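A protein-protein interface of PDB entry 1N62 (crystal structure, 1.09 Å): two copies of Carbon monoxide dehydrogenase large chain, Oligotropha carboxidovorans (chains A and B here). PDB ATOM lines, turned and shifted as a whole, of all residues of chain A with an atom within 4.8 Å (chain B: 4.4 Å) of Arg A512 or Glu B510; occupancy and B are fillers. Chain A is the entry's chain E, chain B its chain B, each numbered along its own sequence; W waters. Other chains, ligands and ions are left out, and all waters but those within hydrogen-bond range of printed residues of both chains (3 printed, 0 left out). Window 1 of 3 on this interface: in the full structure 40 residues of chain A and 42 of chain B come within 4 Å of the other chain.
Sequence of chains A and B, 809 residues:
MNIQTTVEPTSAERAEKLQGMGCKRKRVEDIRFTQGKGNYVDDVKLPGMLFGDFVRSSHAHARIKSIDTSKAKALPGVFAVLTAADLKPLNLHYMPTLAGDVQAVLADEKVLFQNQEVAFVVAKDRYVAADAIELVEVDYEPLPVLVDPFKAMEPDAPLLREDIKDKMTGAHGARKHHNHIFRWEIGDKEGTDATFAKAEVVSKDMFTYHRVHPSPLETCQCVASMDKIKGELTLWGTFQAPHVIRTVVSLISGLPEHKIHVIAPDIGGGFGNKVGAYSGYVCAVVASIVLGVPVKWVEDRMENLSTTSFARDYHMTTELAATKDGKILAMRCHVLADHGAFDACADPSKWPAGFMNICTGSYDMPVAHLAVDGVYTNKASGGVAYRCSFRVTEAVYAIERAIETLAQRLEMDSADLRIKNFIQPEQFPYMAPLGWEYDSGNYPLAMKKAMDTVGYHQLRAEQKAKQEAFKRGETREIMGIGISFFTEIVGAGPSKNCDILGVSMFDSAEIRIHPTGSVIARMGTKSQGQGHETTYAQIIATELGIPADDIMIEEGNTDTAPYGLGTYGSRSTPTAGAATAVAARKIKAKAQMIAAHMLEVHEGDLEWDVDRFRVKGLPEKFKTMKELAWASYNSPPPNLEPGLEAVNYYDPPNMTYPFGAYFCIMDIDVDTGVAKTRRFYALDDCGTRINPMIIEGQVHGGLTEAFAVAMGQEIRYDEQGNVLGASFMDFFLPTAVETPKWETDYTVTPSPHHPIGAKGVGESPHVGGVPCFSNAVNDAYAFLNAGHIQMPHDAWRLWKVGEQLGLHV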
ATOM      1  N   GLU A 510     -11.746 -10.323  27.775  1.00  0.00           N
ATOM      2  CA  GLU A 510     -11.778  -9.614  26.506  1.00  0.00           C
ATOM      3  C   GLU A 510     -11.043  -8.337  26.733  1.00  0.00           C
ATOM      4  O   GLU A 510     -11.311  -7.648  27.677  1.00  0.00           O
ATOM      5  CB  GLU A 510     -13.204  -9.359  26.071  1.00  0.00           C
ATOM      6  CG  GLU A 510     -13.245  -8.526  24.808  1.00  0.00           C
ATOM      7  CD  GLU A 510     -14.537  -8.651  24.053  1.00  0.00           C
ATOM      8  OE1 GLU A 510     -15.596  -8.798  24.673  1.00  0.00           O
ATOM      9  OE2 GLU A 510     -14.466  -8.628  22.803  1.00  0.00           O
ATOM     10  N   ILE A 511     -10.113  -8.046  25.849  1.00  0.00           N
ATOM     11  CA  ILE A 511      -9.250  -6.875  25.972  1.00  0.00           C
ATOM     12  C   ILE A 511      -9.310  -6.118  24.690  1.00  0.00           C
ATOM     13  O   ILE A 511      -9.089  -6.687  23.633  1.00  0.00           O
ATOM     14  CB  ILE A 511      -7.834  -7.303  26.249  1.00  0.00           C
ATOM     15  CG1 ILE A 511      -7.733  -8.196  27.473  1.00  0.00           C
ATOM     16  CG2 ILE A 511      -6.913  -6.114  26.359  1.00  0.00           C
ATOM     17  CD1 ILE A 511      -6.324  -8.726  27.659  1.00  0.00           C
ATOM     18  N   ARG A 512      -9.577  -4.837  24.756  1.00  0.00           N
ATOM     19  CA  ARG A 512      -9.686  -4.020  23.567  1.00  0.00           C
ATOM     20  C   ARG A 512      -8.799  -2.835  23.767  1.00  0.00           C
ATOM     21  O   ARG A 512      -8.920  -2.129  24.750  1.00  0.00           O
ATOM     22  CB  ARG A 512     -11.123  -3.590  23.394  1.00  0.00           C
ATOM     23  CG  ARG A 512     -11.330  -2.629  22.245  1.00  0.00           C
ATOM     24  CD  ARG A 512     -12.782  -2.350  22.000  1.00  0.00           C
ATOM     25  NE  ARG A 512     -13.413  -3.493  21.385  1.00  0.00           N
ATOM     26  CZ  ARG A 512     -14.461  -4.136  21.849  1.00  0.00           C
ATOM     27  NH1 ARG A 512     -15.234  -3.619  22.781  1.00  0.00           N
ATOM     28  NH2 ARG A 512     -14.776  -5.297  21.310  1.00  0.00           N
ATOM     29  N   ILE A 513      -7.906  -2.609  22.825  1.00  0.00           N
ATOM     30  CA  ILE A 513      -7.003  -1.472  22.889  1.00  0.00           C
ATOM     31  C   ILE A 513      -7.573  -0.396  21.997  1.00  0.00           C
ATOM     32  O   ILE A 513      -7.864  -0.625  20.827  1.00  0.00           O
ATOM     33  CB  ILE A 513      -5.570  -1.848  22.394  1.00  0.00           C
ATOM     34  CG1 ILE A 513      -5.150  -3.266  22.819  1.00  0.00           C
ATOM     35  CG2 ILE A 513      -4.580  -0.794  22.824  1.00  0.00           C
ATOM     36  CD1 ILE A 513      -4.933  -3.454  24.333  1.00  0.00           C
ATOM     37  N   HIS A 514      -7.627   0.800  22.527  1.00  0.00           N
ATOM     38  CA  HIS A 514      -8.140   1.932  21.829  1.00  0.00           C
ATOM     39  C   HIS A 514      -7.066   2.538  20.943  1.00  0.00           C
ATOM     40  O   HIS A 514      -5.875   2.292  21.115  1.00  0.00           O
ATOM     41  CB  HIS A 514      -8.599   2.940  22.871  1.00  0.00           C
ATOM     42  CG  HIS A 514      -9.704   2.431  23.700  1.00  0.00           C
ATOM     43  ND1 HIS A 514     -10.686   1.627  23.159  1.00  0.00           N
ATOM     44  CD2 HIS A 514     -10.027   2.647  24.996  1.00  0.00           C
ATOM     45  CE1 HIS A 514     -11.577   1.372  24.112  1.00  0.00           C
ATOM     46  NE2 HIS A 514     -11.165   1.925  25.234  1.00  0.00           N
ATOM     47  N   SER A 518      -4.981   3.223  25.350  1.00  0.00           N
ATOM     48  CA  SER A 518      -5.601   2.770  26.560  1.00  0.00           C
ATOM     49  C   SER A 518      -6.479   1.595  26.243  1.00  0.00           C
ATOM     50  O   SER A 518      -6.624   1.207  25.067  1.00  0.00           O
ATOM     51  CB  SER A 518      -6.371   3.902  27.201  1.00  0.00           C
ATOM     52  OG  SER A 518      -7.294   4.429  26.262  1.00  0.00           O
ATOM     53  N   VAL A 519      -7.003   0.970  27.271  1.00  0.00           N
ATOM     54  CA  VAL A 519      -7.559  -0.355  27.157  1.00  0.00           C
ATOM     55  C   VAL A 519      -8.818  -0.475  27.982  1.00  0.00           C
ATOM     56  O   VAL A 519      -8.852   0.010  29.108  1.00  0.00           O
ATOM     57  CB  VAL A 519      -6.573  -1.331  27.696  1.00  0.00           C
ATOM     58  CG1 VAL A 519      -7.082  -2.746  27.577  1.00  0.00           C
ATOM     59  CG2 VAL A 519      -5.246  -1.151  26.993  1.00  0.00           C
ATOM     60  N   ILE A 520      -9.808  -1.181  27.449  1.00  0.00           N
ATOM     61  CA  ILE A 520     -10.902  -1.700  28.227  1.00  0.00           C
ATOM     62  C   ILE A 520     -10.813  -3.187  28.202  1.00  0.00           C
ATOM     63  O   ILE A 520     -10.714  -3.771  27.140  1.00  0.00           O
ATOM     64  CB  ILE A 520     -12.267  -1.190  27.718  1.00  0.00           C
ATOM     65  CG1 ILE A 520     -13.413  -1.832  28.478  1.00  0.00           C
ATOM     66  CG2 ILE A 520     -12.473  -1.402  26.234  1.00  0.00           C
ATOM     67  CD1 ILE A 520     -13.462  -1.486  29.913  1.00  0.00           C
ATOM     68  N   TYR A 633      -5.333   1.067  13.807  1.00  0.00           N
ATOM     69  CA  TYR A 633      -6.466   1.887  13.387  1.00  0.00           C
ATOM     70  C   TYR A 633      -6.113   2.766  12.217  1.00  0.00           C
ATOM     71  O   TYR A 633      -6.959   3.031  11.388  1.00  0.00           O
ATOM     72  CB  TYR A 633      -6.904   2.735  14.577  1.00  0.00           C
ATOM     73  CG  TYR A 633      -7.566   1.964  15.685  1.00  0.00           C
ATOM     74  CD1 TYR A 633      -6.831   1.425  16.716  1.00  0.00           C
ATOM     75  CD2 TYR A 633      -8.928   1.768  15.691  1.00  0.00           C
ATOM     76  CE1 TYR A 633      -7.407   0.779  17.736  1.00  0.00           C
ATOM     77  CE2 TYR A 633      -9.532   1.081  16.722  1.00  0.00           C
ATOM     78  CZ  TYR A 633      -8.768   0.612  17.767  1.00  0.00           C
ATOM     79  OH  TYR A 633      -9.413  -0.017  18.832  1.00  0.00           O
ATOM     80  N   LEU A 644      -7.267  -3.700  17.496  1.00  0.00           N
ATOM     81  CA  LEU A 644      -6.324  -4.431  18.293  1.00  0.00           C
ATOM     82  C   LEU A 644      -7.034  -4.877  19.556  1.00  0.00           C
ATOM     83  O   LEU A 644      -7.132  -4.143  20.532  1.00  0.00           O
ATOM     84  CB  LEU A 644      -5.111  -3.600  18.571  1.00  0.00           C
ATOM     85  CG  LEU A 644      -3.948  -4.350  19.181  1.00  0.00           C
ATOM     86  CD1 LEU A 644      -3.504  -5.534  18.375  1.00  0.00           C
ATOM     87  CD2 LEU A 644      -2.801  -3.416  19.457  1.00  0.00           C
ATOM     88  N   GLU A 645      -7.526  -6.100  19.545  1.00  0.00           N
ATOM     89  CA  GLU A 645      -8.326  -6.588  20.635  1.00  0.00           C
ATOM     90  C   GLU A 645      -8.321  -8.081  20.578  1.00  0.00           C
ATOM     91  O   GLU A 645      -7.990  -8.670  19.549  1.00  0.00           O
ATOM     92  CB  GLU A 645      -9.718  -6.068  20.566  1.00  0.00           C
ATOM     93  CG  GLU A 645     -10.486  -6.411  19.323  1.00  0.00           C
ATOM     94  CD  GLU A 645     -11.818  -5.771  19.370  1.00  0.00           C
ATOM     95  OE1 GLU A 645     -11.853  -4.531  19.280  1.00  0.00           O
ATOM     96  OE2 GLU A 645     -12.808  -6.442  19.662  1.00  0.00           O
ATOM     97  N   ALA B 509     -18.088  -5.348  13.926  1.00  0.00           N
ATOM     98  CA  ALA B 509     -19.163  -6.080  14.568  1.00  0.00           C
ATOM     99  C   ALA B 509     -18.583  -7.051  15.529  1.00  0.00           C
ATOM    100  O   ALA B 509     -17.557  -7.664  15.264  1.00  0.00           O
ATOM    101  CB  ALA B 509     -19.993  -6.822  13.552  1.00  0.00           C
ATOM    102  N   GLU B 510     -19.274  -7.199  16.649  1.00  0.00           N
ATOM    103  CA  GLU B 510     -18.968  -8.243  17.608  1.00  0.00           C
ATOM    104  C   GLU B 510     -20.241  -8.973  17.912  1.00  0.00           C
ATOM    105  O   GLU B 510     -21.234  -8.358  18.192  1.00  0.00           O
ATOM    106  CB  GLU B 510     -18.407  -7.622  18.906  1.00  0.00           C
ATOM    107  CG  GLU B 510     -18.147  -8.685  19.954  1.00  0.00           C
ATOM    108  CD  GLU B 510     -17.140  -8.290  20.970  1.00  0.00           C
ATOM    109  OE1 GLU B 510     -17.131  -7.141  21.402  1.00  0.00           O
ATOM    110  OE2 GLU B 510     -16.393  -9.157  21.431  1.00  0.00           O
ATOM    111  N   ILE B 511     -20.216 -10.292  17.879  1.00  0.00           N
ATOM    112  CA  ILE B 511     -21.402 -11.102  18.031  1.00  0.00           C
ATOM    113  C   ILE B 511     -21.086 -12.148  19.072  1.00  0.00           C
ATOM    114  O   ILE B 511     -20.100 -12.850  18.934  1.00  0.00           O
ATOM    115  CB  ILE B 511     -21.754 -11.781  16.724  1.00  0.00           C
ATOM    116  CG1 ILE B 511     -21.959 -10.784  15.596  1.00  0.00           C
ATOM    117  CG2 ILE B 511     -22.960 -12.638  16.926  1.00  0.00           C
ATOM    118  CD1 ILE B 511     -22.136 -11.471  14.253  1.00  0.00           C
ATOM    119  N   ARG B 512     -21.931 -12.274  20.082  1.00  0.00           N
ATOM    120  CA  ARG B 512     -21.723 -13.212  21.150  1.00  0.00           C
ATOM    121  C   ARG B 512     -22.970 -14.028  21.328  1.00  0.00           C
ATOM    122  O   ARG B 512     -24.035 -13.514  21.501  1.00  0.00           O
ATOM    123  CB  ARG B 512     -21.384 -12.478  22.443  1.00  0.00           C
ATOM    124  CG  ARG B 512     -21.249 -13.399  23.617  1.00  0.00           C
ATOM    125  CD  ARG B 512     -20.781 -12.656  24.841  1.00  0.00           C
ATOM    126  NE  ARG B 512     -19.374 -12.325  24.703  1.00  0.00           N
ATOM    127  CZ  ARG B 512     -18.841 -11.130  24.840  1.00  0.00           C
ATOM    128  NH1 ARG B 512     -19.570 -10.135  25.283  1.00  0.00           N
ATOM    129  NH2 ARG B 512     -17.617 -10.914  24.367  1.00  0.00           N
ATOM    130  N   ILE B 520     -26.098 -11.387  21.726  1.00  0.00           N
ATOM    131  CA  ILE B 520     -25.856  -9.960  21.806  1.00  0.00           C
ATOM    132  C   ILE B 520     -24.813  -9.606  20.767  1.00  0.00           C
ATOM    133  O   ILE B 520     -23.788 -10.247  20.671  1.00  0.00           O
ATOM    134  CB  ILE B 520     -25.417  -9.517  23.211  1.00  0.00           C
ATOM    135  CG1 ILE B 520     -25.103  -8.017  23.265  1.00  0.00           C
ATOM    136  CG2 ILE B 520     -24.265 -10.295  23.715  1.00  0.00           C
ATOM    137  CD1 ILE B 520     -26.211  -7.144  22.954  1.00  0.00           C
ATOM    138  N   ALA B 521     -25.096  -8.615  19.958  1.00  0.00           N
ATOM    139  CA  ALA B 521     -24.199  -8.191  18.929  1.00  0.00           C
ATOM    140  C   ALA B 521     -24.142  -6.702  18.957  1.00  0.00           C
ATOM    141  O   ALA B 521     -25.141  -6.033  19.161  1.00  0.00           O
ATOM    142  CB  ALA B 521     -24.667  -8.678  17.589  1.00  0.00           C
ATOM    143  N   ARG B 522     -22.955  -6.187  18.721  1.00  0.00           N
ATOM    144  CA  ARG B 522     -22.741  -4.771  18.669  1.00  0.00           C
ATOM    145  C   ARG B 522     -21.914  -4.393  17.450  1.00  0.00           C
ATOM    146  O   ARG B 522     -21.133  -5.169  16.967  1.00  0.00           O
ATOM    147  CB  ARG B 522     -22.041  -4.248  19.910  1.00  0.00           C
ATOM    148  CG  ARG B 522     -22.759  -4.631  21.170  1.00  0.00           C
ATOM    149  CD  ARG B 522     -22.286  -3.869  22.348  1.00  0.00           C
ATOM    150  NE  ARG B 522     -23.024  -4.156  23.555  1.00  0.00           N
ATOM    151  CZ  ARG B 522     -22.782  -5.146  24.365  1.00  0.00           C
ATOM    152  NH1 ARG B 522     -21.712  -5.901  24.188  1.00  0.00           N
ATOM    153  NH2 ARG B 522     -23.479  -5.216  25.480  1.00  0.00           N
ATOM    154  N   THR B 560     -18.621  -0.355  25.030  1.00  0.00           N
ATOM    155  CA  THR B 560     -19.066  -1.699  24.755  1.00  0.00           C
ATOM    156  C   THR B 560     -19.032  -2.058  23.297  1.00  0.00           C
ATOM    157  O   THR B 560     -18.669  -3.172  22.962  1.00  0.00           O
ATOM    158  CB  THR B 560     -20.476  -1.958  25.326  1.00  0.00           C
ATOM    159  OG1 THR B 560     -21.447  -1.172  24.618  1.00  0.00           O
ATOM    160  CG2 THR B 560     -20.599  -1.573  26.825  1.00  0.00           C
ATOM    161  N   ALA B 561     -19.454  -1.181  22.407  1.00  0.00           N
ATOM    162  CA  ALA B 561     -19.455  -1.490  21.005  1.00  0.00           C
ATOM    163  C   ALA B 561     -18.045  -1.499  20.506  1.00  0.00           C
ATOM    164  O   ALA B 561     -17.216  -0.698  20.923  1.00  0.00           O
ATOM    165  CB  ALA B 561     -20.233  -0.461  20.262  1.00  0.00           C
ATOM    166  N   PRO B 562     -17.750  -2.367  19.567  1.00  0.00           N
ATOM    167  CA  PRO B 562     -16.433  -2.321  18.972  1.00  0.00           C
ATOM    168  C   PRO B 562     -16.217  -1.010  18.265  1.00  0.00           C
ATOM    169  O   PRO B 562     -17.158  -0.351  17.889  1.00  0.00           O
ATOM    170  CB  PRO B 562     -16.486  -3.477  17.969  1.00  0.00           C
ATOM    171  CG  PRO B 562     -17.902  -3.561  17.587  1.00  0.00           C
ATOM    172  CD  PRO B 562     -18.680  -3.228  18.831  1.00  0.00           C
ATOM    173  N   GLU B 645     -18.461 -16.795  19.841  1.00  0.00           N
ATOM    174  CA  GLU B 645     -18.528 -15.397  19.600  1.00  0.00           C
ATOM    175  C   GLU B 645     -17.476 -15.026  18.585  1.00  0.00           C
ATOM    176  O   GLU B 645     -16.528 -15.750  18.363  1.00  0.00           O
ATOM    177  CB  GLU B 645     -18.381 -14.634  20.876  1.00  0.00           C
ATOM    178  CG  GLU B 645     -17.088 -14.842  21.613  1.00  0.00           C
ATOM    179  CD  GLU B 645     -17.101 -14.085  22.893  1.00  0.00           C
ATOM    180  OE1 GLU B 645     -17.893 -14.469  23.799  1.00  0.00           O
ATOM    181  OE2 GLU B 645     -16.477 -13.029  22.956  1.00  0.00           O
ATOM    182  N   ALA B 646     -17.617 -13.841  18.014  1.00  0.00           N
ATOM    183  CA  ALA B 646     -16.615 -13.376  17.086  1.00  0.00           C
ATOM    184  C   ALA B 646     -16.700 -11.884  16.928  1.00  0.00           C
ATOM    185  O   ALA B 646     -17.730 -11.289  17.157  1.00  0.00           O
ATOM    186  CB  ALA B 646     -16.729 -14.058  15.726  1.00  0.00           C
ATOM    187  N   VAL B 647     -15.616 -11.324  16.429  1.00  0.00           N
ATOM    188  CA  VAL B 647     -15.505  -9.932  16.064  1.00  0.00           C
ATOM    189  C   VAL B 647     -14.961  -9.884  14.648  1.00  0.00           C
ATOM    190  O   VAL B 647     -14.138 -10.700  14.261  1.00  0.00           O
ATOM    191  CB  VAL B 647     -14.510  -9.241  17.004  1.00  0.00           C
ATOM    192  CG1 VAL B 647     -14.263  -7.824  16.625  1.00  0.00           C
ATOM    193  CG2 VAL B 647     -14.997  -9.273  18.389  1.00  0.00           C
ATOM    194  N   TYR B 649     -13.422  -6.572  12.215  1.00  0.00           N
ATOM    195  CA  TYR B 649     -13.248  -5.207  11.776  1.00  0.00           C
ATOM    196  C   TYR B 649     -13.006  -5.290  10.284  1.00  0.00           C
ATOM    197  O   TYR B 649     -12.050  -5.908   9.845  1.00  0.00           O
ATOM    198  CB  TYR B 649     -12.063  -4.583  12.474  1.00  0.00           C
ATOM    199  CG  TYR B 649     -12.311  -4.127  13.874  1.00  0.00           C
ATOM    200  CD1 TYR B 649     -12.832  -4.967  14.830  1.00  0.00           C
ATOM    201  CD2 TYR B 649     -12.026  -2.847  14.248  1.00  0.00           C
ATOM    202  CE1 TYR B 649     -13.069  -4.502  16.144  1.00  0.00           C
ATOM    203  CE2 TYR B 649     -12.200  -2.396  15.536  1.00  0.00           C
ATOM    204  CZ  TYR B 649     -12.709  -3.244  16.482  1.00  0.00           C
ATOM    205  OH  TYR B 649     -12.944  -2.783  17.754  1.00  0.00           O
HETATM  206  O   HOH W   1     -17.147  -5.359  24.203  1.00  0.00           O
HETATM  207  O   HOH W   2     -15.461  -0.722  22.956  1.00  0.00           O
HETATM  208  O   HOH W   3      -9.732  -2.872  18.439  1.00  0.00           O
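Printed residues of chain B that touch a printed residue of chain A: Glu B510, Arg B512, Thr B560, Ala B561, Pro B562, Val B647 and Tyr B649.
Among the printed residues, Asp or Glu carboxylates within 4 Å of a Lys or Arg side-chain nitrogen of the other chain: Glu A510 with Arg B512 (2.9 Å) and Arg A512 with Glu B510 (3.0 Å).
Glu A510 touches its own counterpart, Glu B510.
Glu A510 touches Arg B512, and with the chains exchanged Arg A512 touches Glu B510.
5 positions are printed for both chains.
Of the 9 pairs that touch across the chains among the printed residues, 3 have their exchanged pair printed and touching as well.
The side-chain carboxylate of Glu B510 sits close to the side-chain carboxylate of Glu A510 (2.4 Å).
The side-chain carboxylate (OE1) of Glu B510 is in salt-bridge range of the guanidinium group (NH2) of Arg A512, 3.0 Å away.
The side-chain carboxylate of Glu A510 lies within salt-bridge range of the guanidinium group of Arg B512, at 2.9 Å.
The backbone carbonyl oxygen (O) of Thr B560 lies within hydrogen-bond range of the guanidinium group (NH1) of Arg A512, 3.5 Å away.
The side-chain hydroxyl (OH) of Tyr B649 sits at hydrogen-bond distance from the side-chain carboxylate (OE1) of Glu A645 (2.6 Å).
Of the printed residues of chain B, Arg A512 touches Glu B510, Thr B560, Ala B561, Pro B562 and Tyr B649.
Ser A518 touches none of the printed residues of chain B.
Printed residues of chain B within 4 Å of Glu A645: Val B647 and Tyr B649.
Glu B510 touches just these residues of chain A: Glu A510 and Arg A512.
Ala B521 touches none of the printed residues of chain A.
Of the printed residues of chain A, Ala B561 touches Arg A512 (3.99 Å).
Of the printed residues of chain A, Pro B562 touches Arg A512 (3.9 Å).
Printed residues of chain A within 4 Å of Val B647: Glu A645 (3.6 Å).
The nearest printed residue of chain A that does not touch Val B647 is Glu A510 (4.5 Å).
O of Ala B561 touches NH1 of Arg A512, 3.99 Å away.
CA of Pro B562 touches CZ of Arg A512, at 3.9 Å.
Arg A512 touches Tyr B649 (NE to OH, 3.7 Å).
Val B647 touches Glu A645 (CG1 to OE2, 3.6 Å).
Water W2 lies within hydrogen-bond range of O of Ala B561 (2.7 Å) and NH1 of Arg A512 (2.9 Å).
Water W3 lies within hydrogen-bond range of the backbone NH of Leu A644 (2.8 Å), the side-chain carboxylate of Glu A645 (2.8 Å), the side-chain hydroxyl of Tyr A633 (2.9 Å) and the side-chain hydroxyl of Tyr B649 (3.3 Å).
Water W1 lies within hydrogen-bond range of the backbone carbonyl oxygen (O) of Thr B560 (2.9 Å), the guanidinium group (NH1) of Arg A512 (3.0 Å) and the side-chain carboxylate (OE1) of Glu B510 (3.3 Å).
The side-chain carboxylate (OE2) of Glu B510 is in salt-bridge range of the guanidinium group (NH2) of Arg B512.
N of Glu B510 is in hydrogen-bond range of O of Arg B522 (2.8 Å).
N of Arg B512 sits at hydrogen-bond distance from O of Ile B520 (2.8 Å).
The side-chain carboxylate (OE1) of Glu B645 is in salt-bridge range of the guanidinium group (NE) of Arg B512, at 2.8 Å.
OE2 of Glu A510 is in salt-bridge range of NH2 of Arg A512 (3.7 Å).
NH2 of Arg A512 is in salt-bridge range of OE2 of Glu A645 (2.8 Å).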
